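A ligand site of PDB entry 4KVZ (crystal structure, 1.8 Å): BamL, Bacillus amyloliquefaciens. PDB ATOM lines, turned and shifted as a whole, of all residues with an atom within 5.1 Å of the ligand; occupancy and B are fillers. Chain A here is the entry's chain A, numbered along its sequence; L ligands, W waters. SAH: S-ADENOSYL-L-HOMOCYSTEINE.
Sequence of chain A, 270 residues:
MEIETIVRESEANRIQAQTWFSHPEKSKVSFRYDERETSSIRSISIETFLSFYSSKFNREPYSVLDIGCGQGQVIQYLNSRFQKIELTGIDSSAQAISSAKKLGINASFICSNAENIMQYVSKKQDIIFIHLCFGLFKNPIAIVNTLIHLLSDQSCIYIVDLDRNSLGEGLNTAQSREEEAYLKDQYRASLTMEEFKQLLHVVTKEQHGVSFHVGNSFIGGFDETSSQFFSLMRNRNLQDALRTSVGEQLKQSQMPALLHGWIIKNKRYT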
ATOM      1  N   GLN A  18      15.047   2.337 -16.910  1.00  0.00           N
ATOM      2  CA  GLN A  18      15.039   3.106 -18.173  1.00  0.00           C
ATOM      3  C   GLN A  18      16.178   2.725 -19.152  1.00  0.00           C
ATOM      4  O   GLN A  18      16.089   3.011 -20.337  1.00  0.00           O
ATOM      5  CB  GLN A  18      14.997   4.614 -17.912  1.00  0.00           C
ATOM      6  CG  GLN A  18      15.231   5.540 -19.120  1.00  0.00           C
ATOM      7  CD  GLN A  18      14.234   5.351 -20.269  1.00  0.00           C
ATOM      8  OE1 GLN A  18      13.234   4.648 -20.154  1.00  0.00           O
ATOM      9  NE2 GLN A  18      14.521   6.003 -21.408  1.00  0.00           N
ATOM     10  N   PHE A  21      15.309   0.901 -22.430  1.00  0.00           N
ATOM     11  CA  PHE A  21      14.668   1.592 -23.551  1.00  0.00           C
ATOM     12  C   PHE A  21      15.613   2.538 -24.291  1.00  0.00           C
ATOM     13  O   PHE A  21      15.266   3.081 -25.327  1.00  0.00           O
ATOM     14  CB  PHE A  21      13.391   2.319 -23.078  1.00  0.00           C
ATOM     15  CG  PHE A  21      12.391   1.379 -22.457  1.00  0.00           C
ATOM     16  CD1 PHE A  21      11.557   0.601 -23.248  1.00  0.00           C
ATOM     17  CD2 PHE A  21      12.317   1.247 -21.074  1.00  0.00           C
ATOM     18  CE1 PHE A  21      10.671  -0.296 -22.674  1.00  0.00           C
ATOM     19  CE2 PHE A  21      11.430   0.360 -20.490  1.00  0.00           C
ATOM     20  CZ  PHE A  21      10.597  -0.405 -21.292  1.00  0.00           C
ATOM     21  N   ASP A  34       7.270  -6.372 -24.627  1.00  0.00           N
ATOM     22  CA  ASP A  34       6.122  -5.468 -24.532  1.00  0.00           C
ATOM     23  C   ASP A  34       5.103  -5.741 -25.644  1.00  0.00           C
ATOM     24  O   ASP A  34       3.888  -5.764 -25.403  1.00  0.00           O
ATOM     25  CB  ASP A  34       6.569  -3.996 -24.584  1.00  0.00           C
ATOM     26  CG  ASP A  34       7.377  -3.574 -23.364  1.00  0.00           C
ATOM     27  OD1 ASP A  34       7.453  -4.347 -22.374  1.00  0.00           O
ATOM     28  OD2 ASP A  34       7.938  -2.454 -23.394  1.00  0.00           O
ATOM     29  N   GLU A  35       5.580  -6.005 -26.854  1.00  0.00           N
ATOM     30  CA  GLU A  35       4.641  -6.249 -27.944  1.00  0.00           C
ATOM     31  C   GLU A  35       3.963  -7.609 -27.847  1.00  0.00           C
ATOM     32  O   GLU A  35       2.771  -7.743 -28.153  1.00  0.00           O
ATOM     33  CB  GLU A  35       5.269  -5.973 -29.306  1.00  0.00           C
ATOM     34  CG  GLU A  35       5.613  -4.495 -29.502  1.00  0.00           C
ATOM     35  CD  GLU A  35       4.424  -3.570 -29.275  1.00  0.00           C
ATOM     36  OE1 GLU A  35       4.305  -2.944 -28.182  1.00  0.00           O
ATOM     37  OE2 GLU A  35       3.585  -3.450 -30.191  1.00  0.00           O
ATOM     38  N   THR A  38       2.063  -7.296 -23.777  1.00  0.00           N
ATOM     39  CA  THR A  38       1.271  -6.137 -23.348  1.00  0.00           C
ATOM     40  C   THR A  38       0.377  -5.506 -24.420  1.00  0.00           C
ATOM     41  O   THR A  38      -0.389  -4.602 -24.128  1.00  0.00           O
ATOM     42  CB  THR A  38       2.148  -5.053 -22.646  1.00  0.00           C
ATOM     43  OG1 THR A  38       2.811  -4.243 -23.621  1.00  0.00           O
ATOM     44  CG2 THR A  38       3.172  -5.711 -21.739  1.00  0.00           C
ATOM     45  N   ARG A  42      -2.898  -3.182 -23.809  1.00  0.00           N
ATOM     46  CA  ARG A  42      -2.974  -1.831 -24.370  1.00  0.00           C
ATOM     47  C   ARG A  42      -4.326  -1.565 -25.050  1.00  0.00           C
ATOM     48  O   ARG A  42      -4.928  -0.510 -24.833  1.00  0.00           O
ATOM     49  CB  ARG A  42      -1.800  -1.626 -25.342  1.00  0.00           C
ATOM     50  CG  ARG A  42      -1.573  -0.202 -25.821  1.00  0.00           C
ATOM     51  CD  ARG A  42      -0.252  -0.122 -26.591  1.00  0.00           C
ATOM     52  NE  ARG A  42      -0.231  -1.047 -27.715  1.00  0.00           N
ATOM     53  CZ  ARG A  42       0.834  -1.761 -28.086  1.00  0.00           C
ATOM     54  NH1 ARG A  42       1.978  -1.680 -27.424  1.00  0.00           N
ATOM     55  NH2 ARG A  42       0.745  -2.582 -29.125  1.00  0.00           N
ATOM     56  N   ASP A  66      -0.535  11.000 -25.857  1.00  0.00           N
ATOM     57  CA  ASP A  66       0.036   9.741 -25.397  1.00  0.00           C
ATOM     58  C   ASP A  66       1.468   9.959 -24.911  1.00  0.00           C
ATOM     59  O   ASP A  66       2.351  10.320 -25.691  1.00  0.00           O
ATOM     60  CB  ASP A  66       0.034   8.701 -26.523  1.00  0.00           C
ATOM     61  CG  ASP A  66       0.312   7.291 -26.002  1.00  0.00           C
ATOM     62  OD1 ASP A  66       0.131   7.064 -24.794  1.00  0.00           O
ATOM     63  OD2 ASP A  66       0.689   6.418 -26.805  1.00  0.00           O
ATOM     64  N   ILE A  67       1.667   9.720 -23.611  1.00  0.00           N
ATOM     65  CA  ILE A  67       2.967   9.930 -22.956  1.00  0.00           C
ATOM     66  C   ILE A  67       3.775   8.631 -22.969  1.00  0.00           C
ATOM     67  O   ILE A  67       3.300   7.601 -22.508  1.00  0.00           O
ATOM     68  CB  ILE A  67       2.788  10.404 -21.492  1.00  0.00           C
ATOM     69  CG1 ILE A  67       1.910  11.668 -21.405  1.00  0.00           C
ATOM     70  CG2 ILE A  67       4.153  10.636 -20.831  1.00  0.00           C
ATOM     71  CD1 ILE A  67       2.474  12.877 -22.132  1.00  0.00           C
ATOM     72  N   GLY A  68       5.006   8.680 -23.476  1.00  0.00           N
ATOM     73  CA  GLY A  68       5.805   7.476 -23.667  1.00  0.00           C
ATOM     74  C   GLY A  68       5.172   6.633 -24.764  1.00  0.00           C
ATOM     75  O   GLY A  68       4.943   5.434 -24.585  1.00  0.00           O
ATOM     76  N   CYS A  69       4.898   7.281 -25.892  1.00  0.00           N
ATOM     77  CA  CYS A  69       4.066   6.703 -26.950  1.00  0.00           C
ATOM     78  C   CYS A  69       4.692   5.562 -27.736  1.00  0.00           C
ATOM     79  O   CYS A  69       4.035   4.965 -28.589  1.00  0.00           O
ATOM     80  CB  CYS A  69       3.606   7.792 -27.919  1.00  0.00           C
ATOM     81  SG  CYS A  69       4.960   8.535 -28.871  1.00  0.00           S
ATOM     82  N   GLY A  70       5.981   5.288 -27.493  1.00  0.00           N
ATOM     83  CA  GLY A  70       6.700   4.247 -28.217  1.00  0.00           C
ATOM     84  C   GLY A  70       6.617   4.479 -29.712  1.00  0.00           C
ATOM     85  O   GLY A  70       6.805   5.608 -30.191  1.00  0.00           O
ATOM     86  N   ILE A  90       4.429  11.638 -27.360  1.00  0.00           N
ATOM     87  CA  ILE A  90       5.768  12.084 -27.011  1.00  0.00           C
ATOM     88  C   ILE A  90       6.538  10.897 -26.452  1.00  0.00           C
ATOM     89  O   ILE A  90       5.998  10.096 -25.697  1.00  0.00           O
ATOM     90  CB  ILE A  90       5.739  13.282 -26.028  1.00  0.00           C
ATOM     91  CG1 ILE A  90       7.167  13.792 -25.729  1.00  0.00           C
ATOM     92  CG2 ILE A  90       4.972  12.941 -24.757  1.00  0.00           C
ATOM     93  CD1 ILE A  90       7.187  15.152 -25.070  1.00  0.00           C
ATOM     94  N   ASP A  91       7.811  10.773 -26.840  1.00  0.00           N
ATOM     95  CA  ASP A  91       8.664   9.694 -26.344  1.00  0.00           C
ATOM     96  C   ASP A  91      10.104  10.175 -26.455  1.00  0.00           C
ATOM     97  O   ASP A  91      10.437  10.852 -27.398  1.00  0.00           O
ATOM     98  CB  ASP A  91       8.469   8.431 -27.192  1.00  0.00           C
ATOM     99  CG  ASP A  91       8.981   7.194 -26.497  1.00  0.00           C
ATOM    100  OD1 ASP A  91      10.199   7.040 -26.346  1.00  0.00           O
ATOM    101  OD2 ASP A  91       8.152   6.337 -26.110  1.00  0.00           O
ATOM    102  N   SER A  92      10.945   9.822 -25.475  1.00  0.00           N
ATOM    103  CA  SER A  92      12.338  10.287 -25.459  1.00  0.00           C
ATOM    104  C   SER A  92      13.274   9.485 -26.386  1.00  0.00           C
ATOM    105  O   SER A  92      14.395   9.920 -26.694  1.00  0.00           O
ATOM    106  CB  SER A  92      12.875  10.314 -24.023  1.00  0.00           C
ATOM    107  OG  SER A  92      12.763   9.040 -23.420  1.00  0.00           O
ATOM    108  N   SER A  93      12.790   8.336 -26.866  1.00  0.00           N
ATOM    109  CA  SER A  93      13.537   7.504 -27.814  1.00  0.00           C
ATOM    110  C   SER A  93      13.414   8.016 -29.256  1.00  0.00           C
ATOM    111  O   SER A  93      12.320   7.998 -29.836  1.00  0.00           O
ATOM    112  CB  SER A  93      13.059   6.050 -27.752  1.00  0.00           C
ATOM    113  OG  SER A  93      13.591   5.300 -28.830  1.00  0.00           O
ATOM    114  N   ALA A  96      12.067   5.266 -31.576  1.00  0.00           N
ATOM    115  CA  ALA A  96      10.613   5.057 -31.421  1.00  0.00           C
ATOM    116  C   ALA A  96       9.831   6.092 -32.208  1.00  0.00           C
ATOM    117  O   ALA A  96       8.881   5.754 -32.910  1.00  0.00           O
ATOM    118  CB  ALA A  96      10.219   5.075 -29.950  1.00  0.00           C
ATOM    119  N   SER A 112      11.205  13.924 -27.111  1.00  0.00           N
ATOM    120  CA  SER A 112      11.762  14.606 -25.949  1.00  0.00           C
ATOM    121  C   SER A 112      11.344  13.892 -24.657  1.00  0.00           C
ATOM    122  O   SER A 112      10.432  13.045 -24.670  1.00  0.00           O
ATOM    123  CB  SER A 112      11.293  16.060 -25.918  1.00  0.00           C
ATOM    124  OG  SER A 112      11.959  16.782 -24.907  1.00  0.00           O
ATOM    125  N   ASN A 113      12.016  14.233 -23.571  1.00  0.00           N
ATOM    126  CA  ASN A 113      11.597  13.864 -22.216  1.00  0.00           C
ATOM    127  C   ASN A 113      10.221  14.471 -21.963  1.00  0.00           C
ATOM    128  O   ASN A 113      10.003  15.637 -22.247  1.00  0.00           O
ATOM    129  CB  ASN A 113      12.609  14.417 -21.203  1.00  0.00           C
ATOM    130  CG  ASN A 113      12.324  13.995 -19.755  1.00  0.00           C
ATOM    131  OD1 ASN A 113      11.220  13.574 -19.390  1.00  0.00           O
ATOM    132  ND2 ASN A 113      13.340  14.149 -18.921  1.00  0.00           N
ATOM    133  N   ALA A 114       9.308  13.655 -21.430  1.00  0.00           N
ATOM    134  CA  ALA A 114       7.964  14.122 -21.090  1.00  0.00           C
ATOM    135  C   ALA A 114       7.990  15.369 -20.196  1.00  0.00           C
ATOM    136  O   ALA A 114       7.064  16.181 -20.253  1.00  0.00           O
ATOM    137  CB  ALA A 114       7.169  13.003 -20.433  1.00  0.00           C
ATOM    138  N   HIS A 131       0.799   4.844 -20.347  1.00  0.00           N
ATOM    139  CA  HIS A 131       0.650   3.397 -20.315  1.00  0.00           C
ATOM    140  C   HIS A 131       1.976   2.664 -20.172  1.00  0.00           C
ATOM    141  O   HIS A 131       2.859   2.771 -21.035  1.00  0.00           O
ATOM    142  CB  HIS A 131      -0.071   2.923 -21.575  1.00  0.00           C
ATOM    143  CG  HIS A 131      -0.543   1.505 -21.508  1.00  0.00           C
ATOM    144  ND1 HIS A 131      -1.682   1.123 -20.833  1.00  0.00           N
ATOM    145  CD2 HIS A 131      -0.021   0.372 -22.040  1.00  0.00           C
ATOM    146  CE1 HIS A 131      -1.844  -0.179 -20.949  1.00  0.00           C
ATOM    147  NE2 HIS A 131      -0.859  -0.658 -21.677  1.00  0.00           N
ATOM    148  N   LEU A 132       2.115   1.958 -19.062  1.00  0.00           N
ATOM    149  CA  LEU A 132       3.276   1.110 -18.770  1.00  0.00           C
ATOM    150  C   LEU A 132       4.602   1.844 -18.948  1.00  0.00           C
ATOM    151  O   LEU A 132       5.506   1.351 -19.622  1.00  0.00           O
ATOM    152  CB  LEU A 132       3.217  -0.198 -19.591  1.00  0.00           C
ATOM    153  CG  LEU A 132       2.009  -1.091 -19.271  1.00  0.00           C
ATOM    154  CD1 LEU A 132       1.961  -2.301 -20.192  1.00  0.00           C
ATOM    155  CD2 LEU A 132       2.044  -1.525 -17.814  1.00  0.00           C
ATOM    156  N   CYS A 133       4.725   3.027 -18.343  1.00  0.00           N
ATOM    157  CA  CYS A 133       5.977   3.779 -18.409  1.00  0.00           C
ATOM    158  C   CYS A 133       6.185   4.777 -17.261  1.00  0.00           C
ATOM    159  O   CYS A 133       7.217   5.422 -17.211  1.00  0.00           O
ATOM    160  CB  CYS A 133       6.119   4.511 -19.746  1.00  0.00           C
ATOM    161  SG  CYS A 133       4.924   5.839 -20.017  1.00  0.00           S
ATOM    162  N   LEU A 136       9.360   4.866 -15.215  1.00  0.00           N
ATOM    163  CA  LEU A 136      10.607   5.181 -15.903  1.00  0.00           C
ATOM    164  C   LEU A 136      11.022   6.633 -15.715  1.00  0.00           C
ATOM    165  O   LEU A 136      12.177   6.989 -15.964  1.00  0.00           O
ATOM    166  CB  LEU A 136      10.487   4.871 -17.408  1.00  0.00           C
ATOM    167  CG  LEU A 136      10.087   3.432 -17.742  1.00  0.00           C
ATOM    168  CD1 LEU A 136       9.833   3.300 -19.234  1.00  0.00           C
ATOM    169  CD2 LEU A 136      11.138   2.429 -17.286  1.00  0.00           C
ATOM    170  N   PHE A 137      10.086   7.465 -15.286  1.00  0.00           N
ATOM    171  CA  PHE A 137      10.334   8.890 -15.150  1.00  0.00           C
ATOM    172  C   PHE A 137      11.211   9.168 -13.931  1.00  0.00           C
ATOM    173  O   PHE A 137      10.992   8.605 -12.859  1.00  0.00           O
ATOM    174  CB  PHE A 137       9.025   9.664 -15.056  1.00  0.00           C
ATOM    175  CG  PHE A 137       8.101   9.437 -16.230  1.00  0.00           C
ATOM    176  CD1 PHE A 137       8.591   9.383 -17.529  1.00  0.00           C
ATOM    177  CD2 PHE A 137       6.735   9.304 -16.028  1.00  0.00           C
ATOM    178  CE1 PHE A 137       7.734   9.180 -18.601  1.00  0.00           C
ATOM    179  CE2 PHE A 137       5.873   9.110 -17.100  1.00  0.00           C
ATOM    180  CZ  PHE A 137       6.371   9.048 -18.391  1.00  0.00           C
HETATM  181  N   SAH L   1       3.198   3.505 -23.726  1.00  0.00           N
HETATM  182  CA  SAH L   1       4.005   2.425 -24.298  1.00  0.00           C
HETATM  183  CB  SAH L   1       5.228   2.162 -23.429  1.00  0.00           C
HETATM  184  CG  SAH L   1       6.417   1.844 -24.325  1.00  0.00           C
HETATM  185  SD  SAH L   1       7.800   1.278 -23.349  1.00  0.00           S
HETATM  186  C   SAH L   1       3.191   1.171 -24.374  1.00  0.00           C
HETATM  187  O   SAH L   1       2.233   0.992 -23.637  1.00  0.00           O
HETATM  188  OXT SAH L   1       3.475   0.283 -25.183  1.00  0.00           O
HETATM  189  C5' SAH L   1       8.192   2.700 -22.376  1.00  0.00           C
HETATM  190  C4' SAH L   1       8.425   3.910 -23.267  1.00  0.00           C
HETATM  191  O4' SAH L   1       8.596   5.074 -22.464  1.00  0.00           O
HETATM  192  C3' SAH L   1       9.678   3.782 -24.131  1.00  0.00           C
HETATM  193  O3' SAH L   1       9.337   3.990 -25.514  1.00  0.00           O
HETATM  194  C2' SAH L   1      10.593   4.885 -23.628  1.00  0.00           C
HETATM  195  O2' SAH L   1      11.418   5.434 -24.661  1.00  0.00           O
HETATM  196  C1' SAH L   1       9.612   5.885 -23.079  1.00  0.00           C
HETATM  197  N9  SAH L   1      10.158   6.816 -22.065  1.00  0.00           N
HETATM  198  C8  SAH L   1      10.924   6.505 -21.006  1.00  0.00           C
HETATM  199  N7  SAH L   1      11.216   7.617 -20.277  1.00  0.00           N
HETATM  200  C5  SAH L   1      10.622   8.653 -20.889  1.00  0.00           C
HETATM  201  C6  SAH L   1      10.524  10.113 -20.678  1.00  0.00           C
HETATM  202  N6  SAH L   1      11.128  10.705 -19.611  1.00  0.00           N
HETATM  203  N1  SAH L   1       9.798  10.835 -21.554  1.00  0.00           N
HETATM  204  C2  SAH L   1       9.178  10.291 -22.620  1.00  0.00           C
HETATM  205  N3  SAH L   1       9.237   8.974 -22.873  1.00  0.00           N
HETATM  206  C4  SAH L   1       9.929   8.128 -22.069  1.00  0.00           C
HETATM  207  O   HOH W   1       6.452  -0.867 -21.074  1.00  0.00           O
HETATM  208  O   HOH W   2       5.523  -0.634 -26.942  1.00  0.00           O
HETATM  209  O   HOH W   3      13.702   6.618 -23.968  1.00  0.00           O
HETATM  210  O   HOH W   4       1.447   5.721 -22.848  1.00  0.00           O
HETATM  211  O   HOH W   5       1.537   4.025 -25.656  1.00  0.00           O
HETATM  212  O   HOH W   6       7.995  -1.349 -25.647  1.00  0.00           O
HETATM  213  O   HOH W   7       1.414  -1.734 -24.119  1.00  0.00           O
HETATM  214  O   HOH W   8      12.726  11.107 -16.745  1.00  0.00           O
HETATM  215  O   HOH W   9       4.270  -1.945 -22.976  1.00  0.00           O
HETATM  216  O   HOH W  10      13.022   8.321 -18.346  1.00  0.00           O
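N of Ser 93 lies within hydrogen-bond range of OD1 of Asp 91 (2.9 Å). The guanidinium group (NH1) of Arg 42 is in salt-bridge range of the side-chain carboxylate (OE1) of Glu 35, at 2.8 Å. OD2 of Asp 91 lies within hydrogen-bond range of N of Gly 70 (2.8 Å). The backbone carbonyl oxygen (O) of Ser 112 is in hydrogen-bond range of the backbone NH (N) of Ser 92 (3.4 Å). The side-chain hydroxyl (OG) of Ser 93 is in hydrogen-bond range of the backbone NH (N) of Ala 96. The backbone NH (N) of Gly 68 is in hydrogen-bond range of the backbone carbonyl oxygen (O) of Ile 90 (2.8 Å). The backbone NH of Ser 112 sits at hydrogen-bond distance from the backbone carbonyl oxygen of Asp 91 (3.2 Å). N of Cys 69 sits at hydrogen-bond distance from OD2 of Asp 91 (3.4 Å).
The backbone NH (N) of Ala 114 sits at hydrogen-bond distance from a nitrogen (N1) of the ligand (2.9 Å). N of the ligand lies within hydrogen-bond range of O of His 131, at 2.8 Å. A nitrogen (N3) of the ligand sits at hydrogen-bond distance from the backbone NH (N) of Ser 92, at 3.2 Å. The backbone carbonyl oxygen of Gly 68 is in hydrogen-bond range of a nitrogen (N) of the ligand (2.7 Å). OD1 of Asp 91 lies within hydrogen-bond range of O2' of the ligand. The guanidinium group (NH1) of Arg 42 is in salt-bridge range of an oxygen (OXT) of the ligand, at 3.3 Å. OD1 of Asn 113 lies within hydrogen-bond range of N6 of the ligand (2.9 Å).
OD2 of Asp 34 lies close to SD of the ligand (3.7 Å). Merely in contact with the ligand: Gln 18, Phe 21, Gly 70, Ser 93, Ser 112, Leu 132, Cys 133, Leu 136 and Phe 137. Hydrophobic or aromatic side chains that line the ligand: Phe 21, Ala 114, His 131, Leu 136 and Phe 137. Within 4 Å of the ligand: Gln 18, Phe 21, Asp 34, Arg 42, Gly 68, Gly 70, Asp 91, Ser 92, Ser 93, Ser 112, Asn 113, Ala 114, His 131, Leu 132, Cys 133, Leu 136 and Phe 137. The nearest printed residue that does not touch the ligand is Ile 67 (4.3 Å).
Water W10 lies within hydrogen-bond range of a nitrogen (N7) of the ligand (2.7 Å) and the backbone carbonyl oxygen of Leu 136 (2.9 Å). Water W2 bridges OXT of the ligand (2.9 Å) and OE1 of Glu 35 (2.9 Å). Water W7 lies within hydrogen-bond range of an oxygen (O) of the ligand, the side-chain hydroxyl (OG1) of Thr 38 and the guanidinium group (NH1) of Arg 42. Water W4 lies within hydrogen-bond range of the backbone carbonyl oxygen of Ile 67, the side-chain carboxylate of Asp 66, the backbone NH of His 131 and a nitrogen (N) of the ligand. Water W9 lies within hydrogen-bond range of the side-chain hydroxyl of Thr 38 (2.8 Å) and an oxygen (OXT) of the ligand (3.2 Å). Water W6 bridges the side-chain carboxylate of Asp 34 and a sulfur (SD) of the ligand.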
